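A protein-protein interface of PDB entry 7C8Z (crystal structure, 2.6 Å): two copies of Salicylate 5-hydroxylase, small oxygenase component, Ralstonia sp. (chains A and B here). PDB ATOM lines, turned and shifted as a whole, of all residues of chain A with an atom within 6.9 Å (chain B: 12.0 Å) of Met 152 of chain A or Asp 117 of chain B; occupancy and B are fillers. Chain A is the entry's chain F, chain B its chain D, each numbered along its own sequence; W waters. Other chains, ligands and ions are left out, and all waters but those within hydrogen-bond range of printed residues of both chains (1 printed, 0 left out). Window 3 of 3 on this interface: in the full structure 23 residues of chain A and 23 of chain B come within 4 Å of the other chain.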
ATOM      1  N   GLU A  45     -13.550  32.539 -24.554  1.00  0.00           N
ATOM      2  CA  GLU A  45     -14.923  32.136 -24.258  1.00  0.00           C
ATOM      3  C   GLU A  45     -15.938  33.122 -24.827  1.00  0.00           C
ATOM      4  O   GLU A  45     -16.984  32.710 -25.340  1.00  0.00           O
ATOM      5  CB  GLU A  45     -15.120  31.966 -22.749  1.00  0.00           C
ATOM      6  CG  GLU A  45     -14.713  33.163 -21.910  1.00  0.00           C
ATOM      7  CD  GLU A  45     -14.843  32.888 -20.429  1.00  0.00           C
ATOM      8  OE1 GLU A  45     -15.715  32.074 -20.058  1.00  0.00           O
ATOM      9  OE2 GLU A  45     -14.068  33.473 -19.637  1.00  0.00           O
ATOM     10  N   PHE A 123       1.989  34.784 -18.756  1.00  0.00           N
ATOM     11  CA  PHE A 123       0.998  35.769 -18.344  1.00  0.00           C
ATOM     12  C   PHE A 123      -0.265  35.678 -19.186  1.00  0.00           C
ATOM     13  O   PHE A 123      -1.380  35.622 -18.650  1.00  0.00           O
ATOM     14  CB  PHE A 123       1.620  37.153 -18.462  1.00  0.00           C
ATOM     15  CG  PHE A 123       0.729  38.268 -18.029  1.00  0.00           C
ATOM     16  CD1 PHE A 123       0.127  38.253 -16.783  1.00  0.00           C
ATOM     17  CD2 PHE A 123       0.532  39.359 -18.855  1.00  0.00           C
ATOM     18  CE1 PHE A 123      -0.671  39.292 -16.382  1.00  0.00           C
ATOM     19  CE2 PHE A 123      -0.264  40.396 -18.460  1.00  0.00           C
ATOM     20  CZ  PHE A 123      -0.867  40.361 -17.222  1.00  0.00           C
ATOM     21  N   TYR A 148      -7.385  35.439 -26.622  1.00  0.00           N
ATOM     22  CA  TYR A 148      -6.446  34.838 -25.679  1.00  0.00           C
ATOM     23  C   TYR A 148      -7.049  33.659 -24.925  1.00  0.00           C
ATOM     24  O   TYR A 148      -8.203  33.705 -24.488  1.00  0.00           O
ATOM     25  CB  TYR A 148      -5.895  35.871 -24.686  1.00  0.00           C
ATOM     26  CG  TYR A 148      -6.891  36.542 -23.768  1.00  0.00           C
ATOM     27  CD1 TYR A 148      -7.519  37.719 -24.141  1.00  0.00           C
ATOM     28  CD2 TYR A 148      -7.162  36.028 -22.505  1.00  0.00           C
ATOM     29  CE1 TYR A 148      -8.420  38.350 -23.297  1.00  0.00           C
ATOM     30  CE2 TYR A 148      -8.062  36.654 -21.652  1.00  0.00           C
ATOM     31  CZ  TYR A 148      -8.689  37.812 -22.057  1.00  0.00           C
ATOM     32  OH  TYR A 148      -9.583  38.444 -21.218  1.00  0.00           O
ATOM     33  N   ASP A 149      -6.234  32.608 -24.764  1.00  0.00           N
ATOM     34  CA  ASP A 149      -6.633  31.443 -23.982  1.00  0.00           C
ATOM     35  C   ASP A 149      -6.595  31.726 -22.485  1.00  0.00           C
ATOM     36  O   ASP A 149      -7.355  31.114 -21.726  1.00  0.00           O
ATOM     37  CB  ASP A 149      -5.720  30.247 -24.290  1.00  0.00           C
ATOM     38  CG  ASP A 149      -5.624  29.925 -25.781  1.00  0.00           C
ATOM     39  OD1 ASP A 149      -6.633  30.034 -26.510  1.00  0.00           O
ATOM     40  OD2 ASP A 149      -4.520  29.550 -26.227  1.00  0.00           O
ATOM     41  N   SER A 150      -5.733  32.649 -22.044  1.00  0.00           N
ATOM     42  CA  SER A 150      -5.454  32.856 -20.619  1.00  0.00           C
ATOM     43  C   SER A 150      -6.564  33.692 -19.975  1.00  0.00           C
ATOM     44  O   SER A 150      -6.365  34.820 -19.515  1.00  0.00           O
ATOM     45  CB  SER A 150      -4.099  33.526 -20.445  1.00  0.00           C
ATOM     46  OG  SER A 150      -3.125  32.910 -21.260  1.00  0.00           O
ATOM     47  N   GLU A 151      -7.748  33.078 -19.898  1.00  0.00           N
ATOM     48  CA  GLU A 151      -8.923  33.793 -19.417  1.00  0.00           C
ATOM     49  C   GLU A 151      -8.772  34.194 -17.956  1.00  0.00           C
ATOM     50  O   GLU A 151      -9.193  35.289 -17.561  1.00  0.00           O
ATOM     51  CB  GLU A 151     -10.176  32.943 -19.623  1.00  0.00           C
ATOM     52  CG  GLU A 151     -10.438  32.623 -21.087  1.00  0.00           C
ATOM     53  CD  GLU A 151     -11.325  31.413 -21.286  1.00  0.00           C
ATOM     54  OE1 GLU A 151     -11.914  31.287 -22.383  1.00  0.00           O
ATOM     55  OE2 GLU A 151     -11.438  30.592 -20.351  1.00  0.00           O
ATOM     56  N   MET A 152      -8.187  33.324 -17.137  1.00  0.00           N
ATOM     57  CA  MET A 152      -7.941  33.641 -15.729  1.00  0.00           C
ATOM     58  C   MET A 152      -6.726  34.554 -15.665  1.00  0.00           C
ATOM     59  O   MET A 152      -5.585  34.103 -15.604  1.00  0.00           O
ATOM     60  CB  MET A 152      -7.747  32.369 -14.915  1.00  0.00           C
ATOM     61  CG  MET A 152      -7.834  32.574 -13.416  1.00  0.00           C
ATOM     62  SD  MET A 152      -9.322  33.455 -12.888  1.00  0.00           S
ATOM     63  CE  MET A 152     -10.601  32.280 -13.319  1.00  0.00           C
ATOM     64  N   ILE A 153      -6.977  35.858 -15.692  1.00  0.00           N
ATOM     65  CA  ILE A 153      -5.895  36.841 -15.835  1.00  0.00           C
ATOM     66  C   ILE A 153      -5.097  36.916 -14.537  1.00  0.00           C
ATOM     67  O   ILE A 153      -5.693  37.066 -13.454  1.00  0.00           O
ATOM     68  CB  ILE A 153      -6.469  38.211 -16.211  1.00  0.00           C
ATOM     69  CG1 ILE A 153      -6.879  38.224 -17.685  1.00  0.00           C
ATOM     70  CG2 ILE A 153      -5.455  39.318 -15.939  1.00  0.00           C
ATOM     71  CD1 ILE A 153      -7.948  39.233 -18.005  1.00  0.00           C
ATOM     72  N   PRO A 154      -3.761  36.840 -14.586  1.00  0.00           N
ATOM     73  CA  PRO A 154      -2.970  37.034 -13.362  1.00  0.00           C
ATOM     74  C   PRO A 154      -3.032  38.468 -12.848  1.00  0.00           C
ATOM     75  O   PRO A 154      -2.082  39.246 -12.962  1.00  0.00           O
ATOM     76  CB  PRO A 154      -1.552  36.635 -13.794  1.00  0.00           C
ATOM     77  CG  PRO A 154      -1.759  35.733 -14.976  1.00  0.00           C
ATOM     78  CD  PRO A 154      -2.957  36.288 -15.687  1.00  0.00           C
ATOM     79  N   ASN A 155      -4.200  38.791 -12.286  1.00  0.00           N
ATOM     80  CA  ASN A 155      -4.592  40.012 -11.582  1.00  0.00           C
ATOM     81  C   ASN A 155      -4.808  41.269 -12.427  1.00  0.00           C
ATOM     82  O   ASN A 155      -5.742  42.026 -12.143  1.00  0.00           O
ATOM     83  CB  ASN A 155      -3.525  40.334 -10.526  1.00  0.00           C
ATOM     84  CG  ASN A 155      -3.977  41.370  -9.500  1.00  0.00           C
ATOM     85  OD1 ASN A 155      -4.977  42.061  -9.673  1.00  0.00           O
ATOM     86  ND2 ASN A 155      -3.210  41.492  -8.425  1.00  0.00           N
ATOM     87  N   ASP B  78     -10.671  16.026 -19.568  1.00  0.00           N
ATOM     88  CA  ASP B  78     -10.860  17.417 -19.195  1.00  0.00           C
ATOM     89  C   ASP B  78     -10.620  18.290 -20.420  1.00  0.00           C
ATOM     90  O   ASP B  78      -9.563  18.170 -21.056  1.00  0.00           O
ATOM     91  CB  ASP B  78      -9.910  17.811 -18.066  1.00  0.00           C
ATOM     92  CG  ASP B  78     -10.545  18.769 -17.065  1.00  0.00           C
ATOM     93  OD1 ASP B  78     -11.648  19.284 -17.336  1.00  0.00           O
ATOM     94  OD2 ASP B  78      -9.938  19.011 -16.002  1.00  0.00           O
ATOM     95  N   PRO B  79     -11.570  19.134 -20.811  1.00  0.00           N
ATOM     96  CA  PRO B  79     -11.314  20.068 -21.912  1.00  0.00           C
ATOM     97  C   PRO B  79     -10.292  21.115 -21.509  1.00  0.00           C
ATOM     98  O   PRO B  79     -10.178  21.488 -20.338  1.00  0.00           O
ATOM     99  CB  PRO B  79     -12.686  20.706 -22.172  1.00  0.00           C
ATOM    100  CG  PRO B  79     -13.669  19.914 -21.375  1.00  0.00           C
ATOM    101  CD  PRO B  79     -12.916  19.306 -20.243  1.00  0.00           C
ATOM    102  N   TYR B  80      -9.528  21.577 -22.494  1.00  0.00           N
ATOM    103  CA  TYR B  80      -8.534  22.611 -22.252  1.00  0.00           C
ATOM    104  C   TYR B  80      -8.193  23.289 -23.568  1.00  0.00           C
ATOM    105  O   TYR B  80      -8.380  22.720 -24.643  1.00  0.00           O
ATOM    106  CB  TYR B  80      -7.275  22.038 -21.594  1.00  0.00           C
ATOM    107  CG  TYR B  80      -6.588  20.949 -22.391  1.00  0.00           C
ATOM    108  CD1 TYR B  80      -5.620  21.259 -23.339  1.00  0.00           C
ATOM    109  CD2 TYR B  80      -6.890  19.608 -22.178  1.00  0.00           C
ATOM    110  CE1 TYR B  80      -4.980  20.265 -24.062  1.00  0.00           C
ATOM    111  CE2 TYR B  80      -6.255  18.606 -22.899  1.00  0.00           C
ATOM    112  CZ  TYR B  80      -5.301  18.943 -23.836  1.00  0.00           C
ATOM    113  OH  TYR B  80      -4.667  17.959 -24.557  1.00  0.00           O
ATOM    114  N   TYR B  81      -7.721  24.526 -23.474  1.00  0.00           N
ATOM    115  CA  TYR B  81      -7.103  25.184 -24.615  1.00  0.00           C
ATOM    116  C   TYR B  81      -5.631  24.802 -24.683  1.00  0.00           C
ATOM    117  O   TYR B  81      -4.983  24.574 -23.658  1.00  0.00           O
ATOM    118  CB  TYR B  81      -7.225  26.707 -24.531  1.00  0.00           C
ATOM    119  CG  TYR B  81      -8.610  27.255 -24.257  1.00  0.00           C
ATOM    120  CD1 TYR B  81      -9.758  26.565 -24.638  1.00  0.00           C
ATOM    121  CD2 TYR B  81      -8.764  28.482 -23.624  1.00  0.00           C
ATOM    122  CE1 TYR B  81     -11.017  27.083 -24.381  1.00  0.00           C
ATOM    123  CE2 TYR B  81     -10.011  29.007 -23.373  1.00  0.00           C
ATOM    124  CZ  TYR B  81     -11.130  28.311 -23.756  1.00  0.00           C
ATOM    125  OH  TYR B  81     -12.361  28.854 -23.487  1.00  0.00           O
ATOM    126  N   GLN B  82      -5.105  24.732 -25.901  1.00  0.00           N
ATOM    127  CA  GLN B  82      -3.677  24.557 -26.120  1.00  0.00           C
ATOM    128  C   GLN B  82      -3.214  25.546 -27.179  1.00  0.00           C
ATOM    129  O   GLN B  82      -3.974  25.939 -28.066  1.00  0.00           O
ATOM    130  CB  GLN B  82      -3.326  23.114 -26.534  1.00  0.00           C
ATOM    131  CG  GLN B  82      -3.849  22.688 -27.899  1.00  0.00           C
ATOM    132  CD  GLN B  82      -3.327  21.321 -28.326  1.00  0.00           C
ATOM    133  OE1 GLN B  82      -2.792  20.565 -27.511  1.00  0.00           O
ATOM    134  NE2 GLN B  82      -3.490  20.995 -29.606  1.00  0.00           N
ATOM    135  N   ILE B 112       1.392  25.312 -24.895  1.00  0.00           N
ATOM    136  CA  ILE B 112       0.940  25.915 -23.652  1.00  0.00           C
ATOM    137  C   ILE B 112      -0.494  25.480 -23.419  1.00  0.00           C
ATOM    138  O   ILE B 112      -1.366  25.717 -24.262  1.00  0.00           O
ATOM    139  CB  ILE B 112       1.055  27.445 -23.700  1.00  0.00           C
ATOM    140  CG1 ILE B 112       2.530  27.856 -23.723  1.00  0.00           C
ATOM    141  CG2 ILE B 112       0.296  28.077 -22.526  1.00  0.00           C
ATOM    142  CD1 ILE B 112       2.762  29.226 -24.294  1.00  0.00           C
ATOM    143  N   ARG B 113      -0.743  24.845 -22.283  1.00  0.00           N
ATOM    144  CA  ARG B 113      -2.076  24.391 -21.931  1.00  0.00           C
ATOM    145  C   ARG B 113      -2.717  25.364 -20.955  1.00  0.00           C
ATOM    146  O   ARG B 113      -2.044  25.922 -20.084  1.00  0.00           O
ATOM    147  CB  ARG B 113      -2.046  22.987 -21.322  1.00  0.00           C
ATOM    148  CG  ARG B 113      -3.419  22.490 -20.915  1.00  0.00           C
ATOM    149  CD  ARG B 113      -3.377  21.123 -20.276  1.00  0.00           C
ATOM    150  NE  ARG B 113      -2.771  21.130 -18.949  1.00  0.00           N
ATOM    151  CZ  ARG B 113      -2.666  20.045 -18.190  1.00  0.00           C
ATOM    152  NH1 ARG B 113      -3.130  18.886 -18.640  1.00  0.00           N
ATOM    153  NH2 ARG B 113      -2.100  20.111 -16.991  1.00  0.00           N
ATOM    154  N   THR B 114      -4.017  25.595 -21.142  1.00  0.00           N
ATOM    155  CA  THR B 114      -4.850  26.359 -20.218  1.00  0.00           C
ATOM    156  C   THR B 114      -6.108  25.539 -19.958  1.00  0.00           C
ATOM    157  O   THR B 114      -6.984  25.448 -20.826  1.00  0.00           O
ATOM    158  CB  THR B 114      -5.202  27.733 -20.773  1.00  0.00           C
ATOM    159  OG1 THR B 114      -4.037  28.342 -21.349  1.00  0.00           O
ATOM    160  CG2 THR B 114      -5.748  28.619 -19.659  1.00  0.00           C
ATOM    161  N   LYS B 115      -6.191  24.919 -18.786  1.00  0.00           N
ATOM    162  CA  LYS B 115      -7.458  24.347 -18.372  1.00  0.00           C
ATOM    163  C   LYS B 115      -8.413  25.476 -17.987  1.00  0.00           C
ATOM    164  O   LYS B 115      -8.002  26.615 -17.759  1.00  0.00           O
ATOM    165  CB  LYS B 115      -7.244  23.333 -17.248  1.00  0.00           C
ATOM    166  CG  LYS B 115      -6.464  22.108 -17.740  1.00  0.00           C
ATOM    167  CD  LYS B 115      -6.448  20.949 -16.756  1.00  0.00           C
ATOM    168  CE  LYS B 115      -6.523  19.616 -17.501  1.00  0.00           C
ATOM    169  NZ  LYS B 115      -6.407  18.432 -16.592  1.00  0.00           N
ATOM    170  N   TYR B 116      -9.701  25.132 -17.874  1.00  0.00           N
ATOM    171  CA  TYR B 116     -10.766  26.104 -18.135  1.00  0.00           C
ATOM    172  C   TYR B 116     -10.598  27.407 -17.357  1.00  0.00           C
ATOM    173  O   TYR B 116     -10.702  28.497 -17.933  1.00  0.00           O
ATOM    174  CB  TYR B 116     -12.138  25.485 -17.858  1.00  0.00           C
ATOM    175  CG  TYR B 116     -12.757  24.888 -19.105  1.00  0.00           C
ATOM    176  CD1 TYR B 116     -12.568  25.487 -20.343  1.00  0.00           C
ATOM    177  CD2 TYR B 116     -13.515  23.727 -19.046  1.00  0.00           C
ATOM    178  CE1 TYR B 116     -13.120  24.951 -21.487  1.00  0.00           C
ATOM    179  CE2 TYR B 116     -14.075  23.180 -20.187  1.00  0.00           C
ATOM    180  CZ  TYR B 116     -13.874  23.799 -21.409  1.00  0.00           C
ATOM    181  OH  TYR B 116     -14.421  23.267 -22.559  1.00  0.00           O
ATOM    182  N   ASP B 117     -10.321  27.332 -16.061  1.00  0.00           N
ATOM    183  CA  ASP B 117     -10.145  28.557 -15.288  1.00  0.00           C
ATOM    184  C   ASP B 117      -8.767  28.616 -14.644  1.00  0.00           C
ATOM    185  O   ASP B 117      -8.587  29.233 -13.591  1.00  0.00           O
ATOM    186  CB  ASP B 117     -11.244  28.698 -14.240  1.00  0.00           C
ATOM    187  CG  ASP B 117     -12.594  28.974 -14.856  1.00  0.00           C
ATOM    188  OD1 ASP B 117     -12.749  30.042 -15.483  1.00  0.00           O
ATOM    189  OD2 ASP B 117     -13.497  28.120 -14.724  1.00  0.00           O
ATOM    190  N   GLY B 118      -7.784  27.970 -15.269  1.00  0.00           N
ATOM    191  CA  GLY B 118      -6.476  27.807 -14.686  1.00  0.00           C
ATOM    192  C   GLY B 118      -5.419  28.701 -15.310  1.00  0.00           C
ATOM    193  O   GLY B 118      -5.649  29.449 -16.255  1.00  0.00           O
ATOM    194  N   ASP B 119      -4.228  28.600 -14.739  1.00  0.00           N
ATOM    195  CA  ASP B 119      -3.083  29.301 -15.282  1.00  0.00           C
ATOM    196  C   ASP B 119      -2.635  28.638 -16.577  1.00  0.00           C
ATOM    197  O   ASP B 119      -2.931  27.466 -16.839  1.00  0.00           O
ATOM    198  CB  ASP B 119      -1.939  29.329 -14.264  1.00  0.00           C
ATOM    199  CG  ASP B 119      -2.283  30.145 -13.024  1.00  0.00           C
ATOM    200  OD1 ASP B 119      -3.018  31.149 -13.150  1.00  0.00           O
ATOM    201  OD2 ASP B 119      -1.825  29.784 -11.921  1.00  0.00           O
ATOM    202  N   SER B 120      -1.971  29.427 -17.416  1.00  0.00           N
ATOM    203  CA  SER B 120      -1.347  28.914 -18.624  1.00  0.00           C
ATOM    204  C   SER B 120       0.012  28.316 -18.268  1.00  0.00           C
ATOM    205  O   SER B 120       0.856  28.988 -17.663  1.00  0.00           O
ATOM    206  CB  SER B 120      -1.206  30.028 -19.655  1.00  0.00           C
ATOM    207  OG  SER B 120      -2.474  30.428 -20.147  1.00  0.00           O
ATOM    208  N   THR B 121       0.217  27.049 -18.618  1.00  0.00           N
ATOM    209  CA  THR B 121       1.421  26.333 -18.229  1.00  0.00           C
ATOM    210  C   THR B 121       2.079  25.723 -19.458  1.00  0.00           C
ATOM    211  O   THR B 121       1.431  25.465 -20.471  1.00  0.00           O
ATOM    212  CB  THR B 121       1.112  25.236 -17.198  1.00  0.00           C
ATOM    213  OG1 THR B 121       0.270  24.239 -17.792  1.00  0.00           O
ATOM    214  CG2 THR B 121       0.407  25.824 -15.985  1.00  0.00           C
HETATM  215  O   HOH W   1      -3.344  27.766 -23.700  1.00  0.00           O
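The side-chain hydroxyl (OG) of Ser 120 of chain B lies within hydrogen-bond range of the side-chain hydroxyl (OG) of Ser 150 of chain A, 2.8 Å away. O of Tyr 116 of chain B sits close to OE2 of Glu 151 of chain A, at 3.3 Å. OE1 of Glu 151 of chain A lies within hydrogen-bond range of OH of Tyr 81 of chain B (2.7 Å).
The side-chain hydroxyl (OG1) of Thr 114 of chain B lies within hydrogen-bond range of the side-chain hydroxyl (OG) of Ser 120 of chain B (2.9 Å). N of Glu 45 of chain A is in hydrogen-bond range of OE1 of Glu 151 of chain A, at 3.0 Å. O of Tyr 81 of chain B lies within hydrogen-bond range of N of Thr 114 of chain B (2.9 Å).
Tyr 81 of chain B touches Asp 149 of chain A. Asp 149 of chain A touches Thr 114 of chain B (O to CG2, 3.6 Å). O of Asp 117 of chain B touches CG of Met 152 of chain A, 3.4 Å away. CB of Met 152 of chain A touches O of Gly 118 of chain B, 3.8 Å away.
Ser 150 of chain A touches just one residue of chain B: Ser 120 (2.8 Å). Met 152 of chain A touches two residues of chain B. No residue of chain B comes within 4 Å of Ile 153 of chain A. Pro 154 of chain A touches none of the printed residues of chain B. Printed residues of chain A within 4 Å of Tyr 81 of chain B: Asp 149 and Glu 151. Gln 82 of chain B touches none of the printed residues of chain A. Printed residues of chain A within 4 Å of Tyr 116 of chain B: Glu 151. Asp 117 of chain B touches just one residue of chain A: Met 152 (3.4 Å). The nearest printed residue of chain B that does not touch Asp 149 of chain A is Gln 82 of chain B (4.1 Å).
Hydrophobic or aromatic side chains of chain A that line the printed part of chain B: Met 152. Hydrophobic or aromatic side chains of chain B that line the printed part of chain A: Tyr 81. Among the printed residues, no Asp or Glu carboxylate lies within 4 Å of a Lys or Arg side-chain nitrogen of the other chain.
No position is printed for both chains. Of the 7 pairs that touch across the chains among the printed residues, none has its exchanged pair printed and touching as well.
Water W1 lies within hydrogen-bond range of OG1 of Thr 114 of chain B, O of Ile 112 of chain B and OD2 of Asp 149 of chain A.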
